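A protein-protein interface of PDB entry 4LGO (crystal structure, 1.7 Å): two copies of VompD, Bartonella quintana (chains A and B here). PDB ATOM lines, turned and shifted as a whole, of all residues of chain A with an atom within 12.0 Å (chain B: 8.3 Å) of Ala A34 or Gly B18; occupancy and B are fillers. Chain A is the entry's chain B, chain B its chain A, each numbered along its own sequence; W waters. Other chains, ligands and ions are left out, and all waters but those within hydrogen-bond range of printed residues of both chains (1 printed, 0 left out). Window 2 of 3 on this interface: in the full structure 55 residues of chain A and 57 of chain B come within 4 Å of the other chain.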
ATOM      1  N   ALA A  19       0.276 -23.654  25.945  1.00  0.00           N
ATOM      2  CA  ALA A  19       0.997 -22.729  24.999  1.00  0.00           C
ATOM      3  C   ALA A  19       0.132 -21.645  24.386  1.00  0.00           C
ATOM      4  O   ALA A  19      -1.060 -21.834  24.122  1.00  0.00           O
ATOM      5  CB  ALA A  19       1.641 -23.514  23.869  1.00  0.00           C
ATOM      6  N   TRP A  20       0.771 -20.518  24.108  1.00  0.00           N
ATOM      7  CA  TRP A  20       0.126 -19.409  23.409  1.00  0.00           C
ATOM      8  C   TRP A  20       0.931 -19.152  22.150  1.00  0.00           C
ATOM      9  O   TRP A  20       1.998 -19.735  21.983  1.00  0.00           O
ATOM     10  CB  TRP A  20       0.014 -18.170  24.300  1.00  0.00           C
ATOM     11  CG  TRP A  20       1.321 -17.632  24.832  1.00  0.00           C
ATOM     12  CD1 TRP A  20       2.051 -18.111  25.888  1.00  0.00           C
ATOM     13  CD2 TRP A  20       2.013 -16.492  24.351  1.00  0.00           C
ATOM     14  NE1 TRP A  20       3.169 -17.331  26.083  1.00  0.00           N
ATOM     15  CE2 TRP A  20       3.172 -16.334  25.142  1.00  0.00           C
ATOM     16  CE3 TRP A  20       1.770 -15.575  23.320  1.00  0.00           C
ATOM     17  CZ2 TRP A  20       4.082 -15.296  24.921  1.00  0.00           C
ATOM     18  CZ3 TRP A  20       2.676 -14.568  23.093  1.00  0.00           C
ATOM     19  CH2 TRP A  20       3.821 -14.430  23.885  1.00  0.00           C
ATOM     20  N   LYS A  21       0.404 -18.315  21.251  1.00  0.00           N
ATOM     21  CA  LYS A  21       1.021 -18.121  19.942  1.00  0.00           C
ATOM     22  C   LYS A  21       1.337 -16.650  19.724  1.00  0.00           C
ATOM     23  O   LYS A  21       0.531 -15.799  20.075  1.00  0.00           O
ATOM     24  CB  LYS A  21       0.078 -18.604  18.839  1.00  0.00           C
ATOM     25  CG  LYS A  21      -0.097 -20.117  18.785  1.00  0.00           C
ATOM     26  CD  LYS A  21      -1.151 -20.519  17.754  1.00  0.00           C
ATOM     27  CE  LYS A  21      -1.200 -22.027  17.531  1.00  0.00           C
ATOM     28  NZ  LYS A  21      -0.058 -22.555  16.720  1.00  0.00           N
ATOM     29  N   LEU A  22       2.504 -16.368  19.149  1.00  0.00           N
ATOM     30  CA  LEU A  22       2.922 -14.982  18.865  1.00  0.00           C
ATOM     31  C   LEU A  22       3.052 -14.814  17.359  1.00  0.00           C
ATOM     32  O   LEU A  22       3.878 -15.487  16.723  1.00  0.00           O
ATOM     33  CB  LEU A  22       4.257 -14.672  19.562  1.00  0.00           C
ATOM     34  CG  LEU A  22       4.873 -13.290  19.312  1.00  0.00           C
ATOM     35  CD1 LEU A  22       3.911 -12.188  19.716  1.00  0.00           C
ATOM     36  CD2 LEU A  22       6.196 -13.142  20.050  1.00  0.00           C
ATOM     37  N   ILE A  30       4.616 -18.166  16.168  1.00  0.00           N
ATOM     38  CA  ILE A  30       5.633 -18.770  17.024  1.00  0.00           C
ATOM     39  C   ILE A  30       4.889 -19.389  18.207  1.00  0.00           C
ATOM     40  O   ILE A  30       4.111 -18.714  18.887  1.00  0.00           O
ATOM     41  CB  ILE A  30       6.643 -17.705  17.519  1.00  0.00           C
ATOM     42  CG1 ILE A  30       7.464 -17.148  16.349  1.00  0.00           C
ATOM     43  CG2 ILE A  30       7.583 -18.285  18.574  1.00  0.00           C
ATOM     44  CD1 ILE A  30       8.045 -15.774  16.604  1.00  0.00           C
ATOM     45  N   ASP A  31       5.092 -20.684  18.420  1.00  0.00           N
ATOM     46  CA  ASP A  31       4.458 -21.391  19.529  1.00  0.00           C
ATOM     47  C   ASP A  31       5.281 -21.128  20.792  1.00  0.00           C
ATOM     48  O   ASP A  31       6.471 -21.406  20.805  1.00  0.00           O
ATOM     49  CB  ASP A  31       4.421 -22.893  19.256  1.00  0.00           C
ATOM     50  CG  ASP A  31       3.439 -23.265  18.153  1.00  0.00           C
ATOM     51  OD1 ASP A  31       2.368 -22.632  18.078  1.00  0.00           O
ATOM     52  OD2 ASP A  31       3.732 -24.205  17.377  1.00  0.00           O
ATOM     53  N   VAL A  32       4.637 -20.606  21.835  1.00  0.00           N
ATOM     54  CA  VAL A  32       5.328 -20.302  23.084  1.00  0.00           C
ATOM     55  C   VAL A  32       4.866 -21.299  24.151  1.00  0.00           C
ATOM     56  O   VAL A  32       3.828 -21.127  24.799  1.00  0.00           O
ATOM     57  CB  VAL A  32       5.116 -18.831  23.516  1.00  0.00           C
ATOM     58  CG1 VAL A  32       5.892 -18.527  24.784  1.00  0.00           C
ATOM     59  CG2 VAL A  32       5.555 -17.898  22.401  1.00  0.00           C
ATOM     60  N   ASN A  33       5.655 -22.351  24.306  1.00  0.00           N
ATOM     61  CA  ASN A  33       5.360 -23.444  25.239  1.00  0.00           C
ATOM     62  C   ASN A  33       5.866 -23.156  26.657  1.00  0.00           C
ATOM     63  O   ASN A  33       6.579 -22.191  26.886  1.00  0.00           O
ATOM     64  CB  ASN A  33       5.997 -24.734  24.713  1.00  0.00           C
ATOM     65  CG  ASN A  33       5.422 -25.155  23.367  1.00  0.00           C
ATOM     66  OD1 ASN A  33       4.215 -25.309  23.225  1.00  0.00           O
ATOM     67  ND2 ASN A  33       6.286 -25.336  22.369  1.00  0.00           N
ATOM     68  N   ALA A  34       5.493 -23.999  27.613  1.00  0.00           N
ATOM     69  CA  ALA A  34       6.098 -23.932  28.945  1.00  0.00           C
ATOM     70  C   ALA A  34       7.610 -24.080  28.791  1.00  0.00           C
ATOM     71  O   ALA A  34       8.084 -24.952  28.054  1.00  0.00           O
ATOM     72  CB  ALA A  34       5.542 -25.021  29.850  1.00  0.00           C
ATOM     73  N   GLY A  35       8.362 -23.208  29.458  1.00  0.00           N
ATOM     74  CA  GLY A  35       9.819 -23.218  29.387  1.00  0.00           C
ATOM     75  C   GLY A  35      10.427 -22.516  28.177  1.00  0.00           C
ATOM     76  O   GLY A  35      11.647 -22.387  28.100  1.00  0.00           O
ATOM     77  N   SER A  36       9.603 -22.047  27.232  1.00  0.00           N
ATOM     78  CA  SER A  36      10.120 -21.362  26.050  1.00  0.00           C
ATOM     79  C   SER A  36      10.632 -19.975  26.414  1.00  0.00           C
ATOM     80  O   SER A  36      10.121 -19.352  27.350  1.00  0.00           O
ATOM     81  CB  SER A  36       9.042 -21.189  24.967  1.00  0.00           C
ATOM     82  OG  SER A  36       8.634 -22.430  24.453  1.00  0.00           O
ATOM     83  N   THR A  37      11.594 -19.507  25.615  1.00  0.00           N
ATOM     84  CA  THR A  37      12.126 -18.161  25.686  1.00  0.00           C
ATOM     85  C   THR A  37      11.744 -17.380  24.435  1.00  0.00           C
ATOM     86  O   THR A  37      11.949 -17.846  23.296  1.00  0.00           O
ATOM     87  CB  THR A  37      13.653 -18.182  25.815  1.00  0.00           C
ATOM     88  OG1 THR A  37      14.014 -18.840  27.043  1.00  0.00           O
ATOM     89  CG2 THR A  37      14.230 -16.768  25.794  1.00  0.00           C
ATOM     90  N   VAL A  38      11.151 -16.214  24.657  1.00  0.00           N
ATOM     91  CA  VAL A  38      10.912 -15.237  23.600  1.00  0.00           C
ATOM     92  C   VAL A  38      11.973 -14.140  23.742  1.00  0.00           C
ATOM     93  O   VAL A  38      12.180 -13.615  24.853  1.00  0.00           O
ATOM     94  CB  VAL A  38       9.496 -14.637  23.740  1.00  0.00           C
ATOM     95  CG1 VAL A  38       9.290 -13.500  22.756  1.00  0.00           C
ATOM     96  CG2 VAL A  38       8.445 -15.720  23.545  1.00  0.00           C
ATOM     97  N   VAL B  17      -1.827 -21.410  30.580  1.00  0.00           N
ATOM     98  CA  VAL B  17      -0.595 -21.204  29.765  1.00  0.00           C
ATOM     99  C   VAL B  17       0.624 -21.654  30.547  1.00  0.00           C
ATOM    100  O   VAL B  17       0.686 -21.479  31.763  1.00  0.00           O
ATOM    101  CB  VAL B  17      -0.412 -19.711  29.369  1.00  0.00           C
ATOM    102  N   GLY B  18       1.591 -22.229  29.839  1.00  0.00           N
ATOM    103  CA  GLY B  18       2.883 -22.582  30.438  1.00  0.00           C
ATOM    104  C   GLY B  18       3.672 -21.353  30.878  1.00  0.00           C
ATOM    105  O   GLY B  18       3.441 -20.246  30.361  1.00  0.00           O
ATOM    106  N   ALA B  19       4.581 -21.534  31.834  1.00  0.00           N
ATOM    107  CA  ALA B  19       5.497 -20.454  32.242  1.00  0.00           C
ATOM    108  C   ALA B  19       6.536 -20.235  31.149  1.00  0.00           C
ATOM    109  O   ALA B  19       7.091 -21.189  30.619  1.00  0.00           O
ATOM    110  CB  ALA B  19       6.181 -20.800  33.556  1.00  0.00           C
ATOM    111  N   TRP B  20       6.811 -18.983  30.801  1.00  0.00           N
ATOM    112  CA  TRP B  20       7.722 -18.728  29.709  1.00  0.00           C
ATOM    113  C   TRP B  20       8.648 -17.598  30.141  1.00  0.00           C
ATOM    114  O   TRP B  20       8.468 -17.053  31.232  1.00  0.00           O
ATOM    115  CB  TRP B  20       6.940 -18.423  28.416  1.00  0.00           C
ATOM    116  CG  TRP B  20       6.001 -17.258  28.514  1.00  0.00           C
ATOM    117  CD1 TRP B  20       4.766 -17.230  29.099  1.00  0.00           C
ATOM    118  CD2 TRP B  20       6.231 -15.949  28.004  1.00  0.00           C
ATOM    119  NE1 TRP B  20       4.211 -15.981  28.987  1.00  0.00           N
ATOM    120  CE2 TRP B  20       5.095 -15.168  28.324  1.00  0.00           C
ATOM    121  CE3 TRP B  20       7.287 -15.356  27.302  1.00  0.00           C
ATOM    122  CZ2 TRP B  20       4.988 -13.820  27.956  1.00  0.00           C
ATOM    123  CZ3 TRP B  20       7.183 -14.030  26.958  1.00  0.00           C
ATOM    124  CH2 TRP B  20       6.039 -13.274  27.283  1.00  0.00           C
ATOM    125  N   LYS B  21       9.651 -17.291  29.322  1.00  0.00           N
ATOM    126  CA  LYS B  21      10.626 -16.237  29.655  1.00  0.00           C
ATOM    127  C   LYS B  21      10.757 -15.225  28.525  1.00  0.00           C
ATOM    128  O   LYS B  21      10.714 -15.573  27.341  1.00  0.00           O
ATOM    129  CB  LYS B  21      12.008 -16.839  29.899  1.00  0.00           C
ATOM    130  CG  LYS B  21      12.084 -17.760  31.090  1.00  0.00           C
ATOM    131  CD  LYS B  21      13.133 -18.841  30.876  1.00  0.00           C
ATOM    132  CE  LYS B  21      12.619 -19.911  29.938  1.00  0.00           C
ATOM    133  NZ  LYS B  21      13.419 -21.159  30.067  1.00  0.00           N
ATOM    134  N   VAL B  32       7.642 -15.240  33.223  1.00  0.00           N
ATOM    135  CA  VAL B  32       6.204 -14.941  33.174  1.00  0.00           C
ATOM    136  C   VAL B  32       5.389 -16.205  33.524  1.00  0.00           C
ATOM    137  O   VAL B  32       5.450 -17.231  32.824  1.00  0.00           O
ATOM    138  CB  VAL B  32       5.805 -14.399  31.791  1.00  0.00           C
ATOM    139  CG1 VAL B  32       4.340 -13.955  31.779  1.00  0.00           C
ATOM    140  CG2 VAL B  32       6.723 -13.247  31.367  1.00  0.00           C
ATOM    141  N   ASN B  33       4.640 -16.131  34.621  1.00  0.00           N
ATOM    142  CA  ASN B  33       3.851 -17.283  35.087  1.00  0.00           C
ATOM    143  C   ASN B  33       2.369 -17.073  34.805  1.00  0.00           C
ATOM    144  O   ASN B  33       1.944 -15.970  34.438  1.00  0.00           O
ATOM    145  CB  ASN B  33       4.072 -17.494  36.581  1.00  0.00           C
ATOM    146  CG  ASN B  33       5.523 -17.815  36.913  1.00  0.00           C
ATOM    147  OD1 ASN B  33       6.043 -18.857  36.510  1.00  0.00           O
ATOM    148  ND2 ASN B  33       6.180 -16.925  37.639  1.00  0.00           N
ATOM    149  N   ALA B  34       1.568 -18.119  34.983  1.00  0.00           N
ATOM    150  CA  ALA B  34       0.130 -17.927  34.990  1.00  0.00           C
ATOM    151  C   ALA B  34      -0.159 -16.908  36.082  1.00  0.00           C
ATOM    152  O   ALA B  34       0.402 -16.981  37.166  1.00  0.00           O
ATOM    153  CB  ALA B  34      -0.586 -19.238  35.280  1.00  0.00           C
ATOM    154  N   GLY B  35      -0.999 -15.928  35.785  1.00  0.00           N
ATOM    155  CA  GLY B  35      -1.309 -14.879  36.751  1.00  0.00           C
ATOM    156  C   GLY B  35      -0.410 -13.656  36.677  1.00  0.00           C
ATOM    157  O   GLY B  35      -0.689 -12.655  37.338  1.00  0.00           O
HETATM  158  O   HOH W   1      14.195 -21.543  26.750  1.00  0.00           O
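The backbone carbonyl oxygen (O) of Trp B20 lies within hydrogen-bond range of the backbone NH (N) of Val B32 (2.8 Å).
N of Val A32 lies within hydrogen-bond range of O of Trp A20 (2.8 Å).
N of Asn A33 lies within hydrogen-bond range of OG of Ser A36, 3.0 Å away.
Water W1 lies within hydrogen-bond range of OG1 of Thr A37 (2.7 Å), O of Gly A35 (3.0 Å) and NZ of Lys B21 (3.4 Å).
Among the printed residues, pairs that only touch across the chains: Ala A34 with Ala B19 (3.4 Å), Thr A37 with Lys B21 (3.4 Å), Ser A36 with Trp B20 (3.4 Å), Ala A34 with Gly B18 (3.7 Å), Val A32 with Trp B20 (3.8 Å), Asn A33 with Ala B19 (3.9 Å) and Val A38 with Trp B20 (3.9 Å).
Printed residues of chain A that touch a printed residue of chain B: Trp A20, Val A32, Asn A33, Ala A34, Gly A35, Ser A36, Thr A37 and Val A38.
Hydrophobic or aromatic side chains of chain A that line the printed part of chain B: Trp A20, Val A32, Ala A34 and Val A38.
Along chain A the printed residues that touch a printed residue of chain B span positions 20 to 38.
Of the 9 printed residues of chain B, 4 touch a printed residue of chain A.
Among the printed residues, no Asp or Glu carboxylate lies within 4 Å of a Lys or Arg side-chain nitrogen of the other chain.
Of chain B, only Gly B18 (3.7 Å) and Ala B19 (3.4 Å) come within 4 Å of Ala A34.
Gly B18 touches just one residue of chain A: Ala A34.
No residue of chain A comes within 4 Å of Val B17.
Ala B19 touches just these residues of chain A: Asn A33, Ala A34 and Gly A35.
Val B32 touches none of the printed residues of chain A.
Of the printed residues of chain B, Val A32 touches Trp B20 (3.8 Å).
Printed residues of chain A within 4 Å of Lys B21: Gly A35, Ser A36, Thr A37 and Val A38.
Printed residues of chain B within 4 Å of Val A38: Trp B20 and Lys B21.
Of the printed residues of chain B, Gly A35 touches Ala B19 and Lys B21.
Of the printed residues of chain B, Thr A37 touches Lys B21 (3.4 Å).
The nearest residue of chain A that does not touch Gly B18 is Ala A19 (4.4 Å).
The nearest printed residue of chain B that does not touch Trp A20 is Val B17 (4.6 Å).
Asn A33 touches Ala B19, but with the chains exchanged Ala A19 does not touch Asn B33 (11.2 Å).
Ala A34 touches Ala B19, but with the chains exchanged Ala A19 does not touch Ala B34 (10.4 Å).
Gly A35 touches Ala B19, but with the chains exchanged Ala A19 does not touch Gly B35 (12.6 Å).
Gly A35 touches Lys B21, but with the chains exchanged Lys A21 does not touch Gly B35 (14.8 Å).
The backbone NH of Gly A35 is in hydrogen-bond range of the backbone carbonyl oxygen of Ala B19, 2.7 Å away.
The side-chain amino group (NZ) of Lys B21 lies within hydrogen-bond range of the backbone carbonyl oxygen (O) of Gly A35 (2.9 Å).
The backbone NH (N) of Lys B21 sits at hydrogen-bond distance from the backbone carbonyl oxygen (O) of Ser A36 (2.9 Å).
N of Val A38 sits at hydrogen-bond distance from O of Lys B21.
The indole nitrogen (NE1) of Trp A20 lies close to the indole nitrogen (NE1) of Trp B20, 3.4 Å away.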
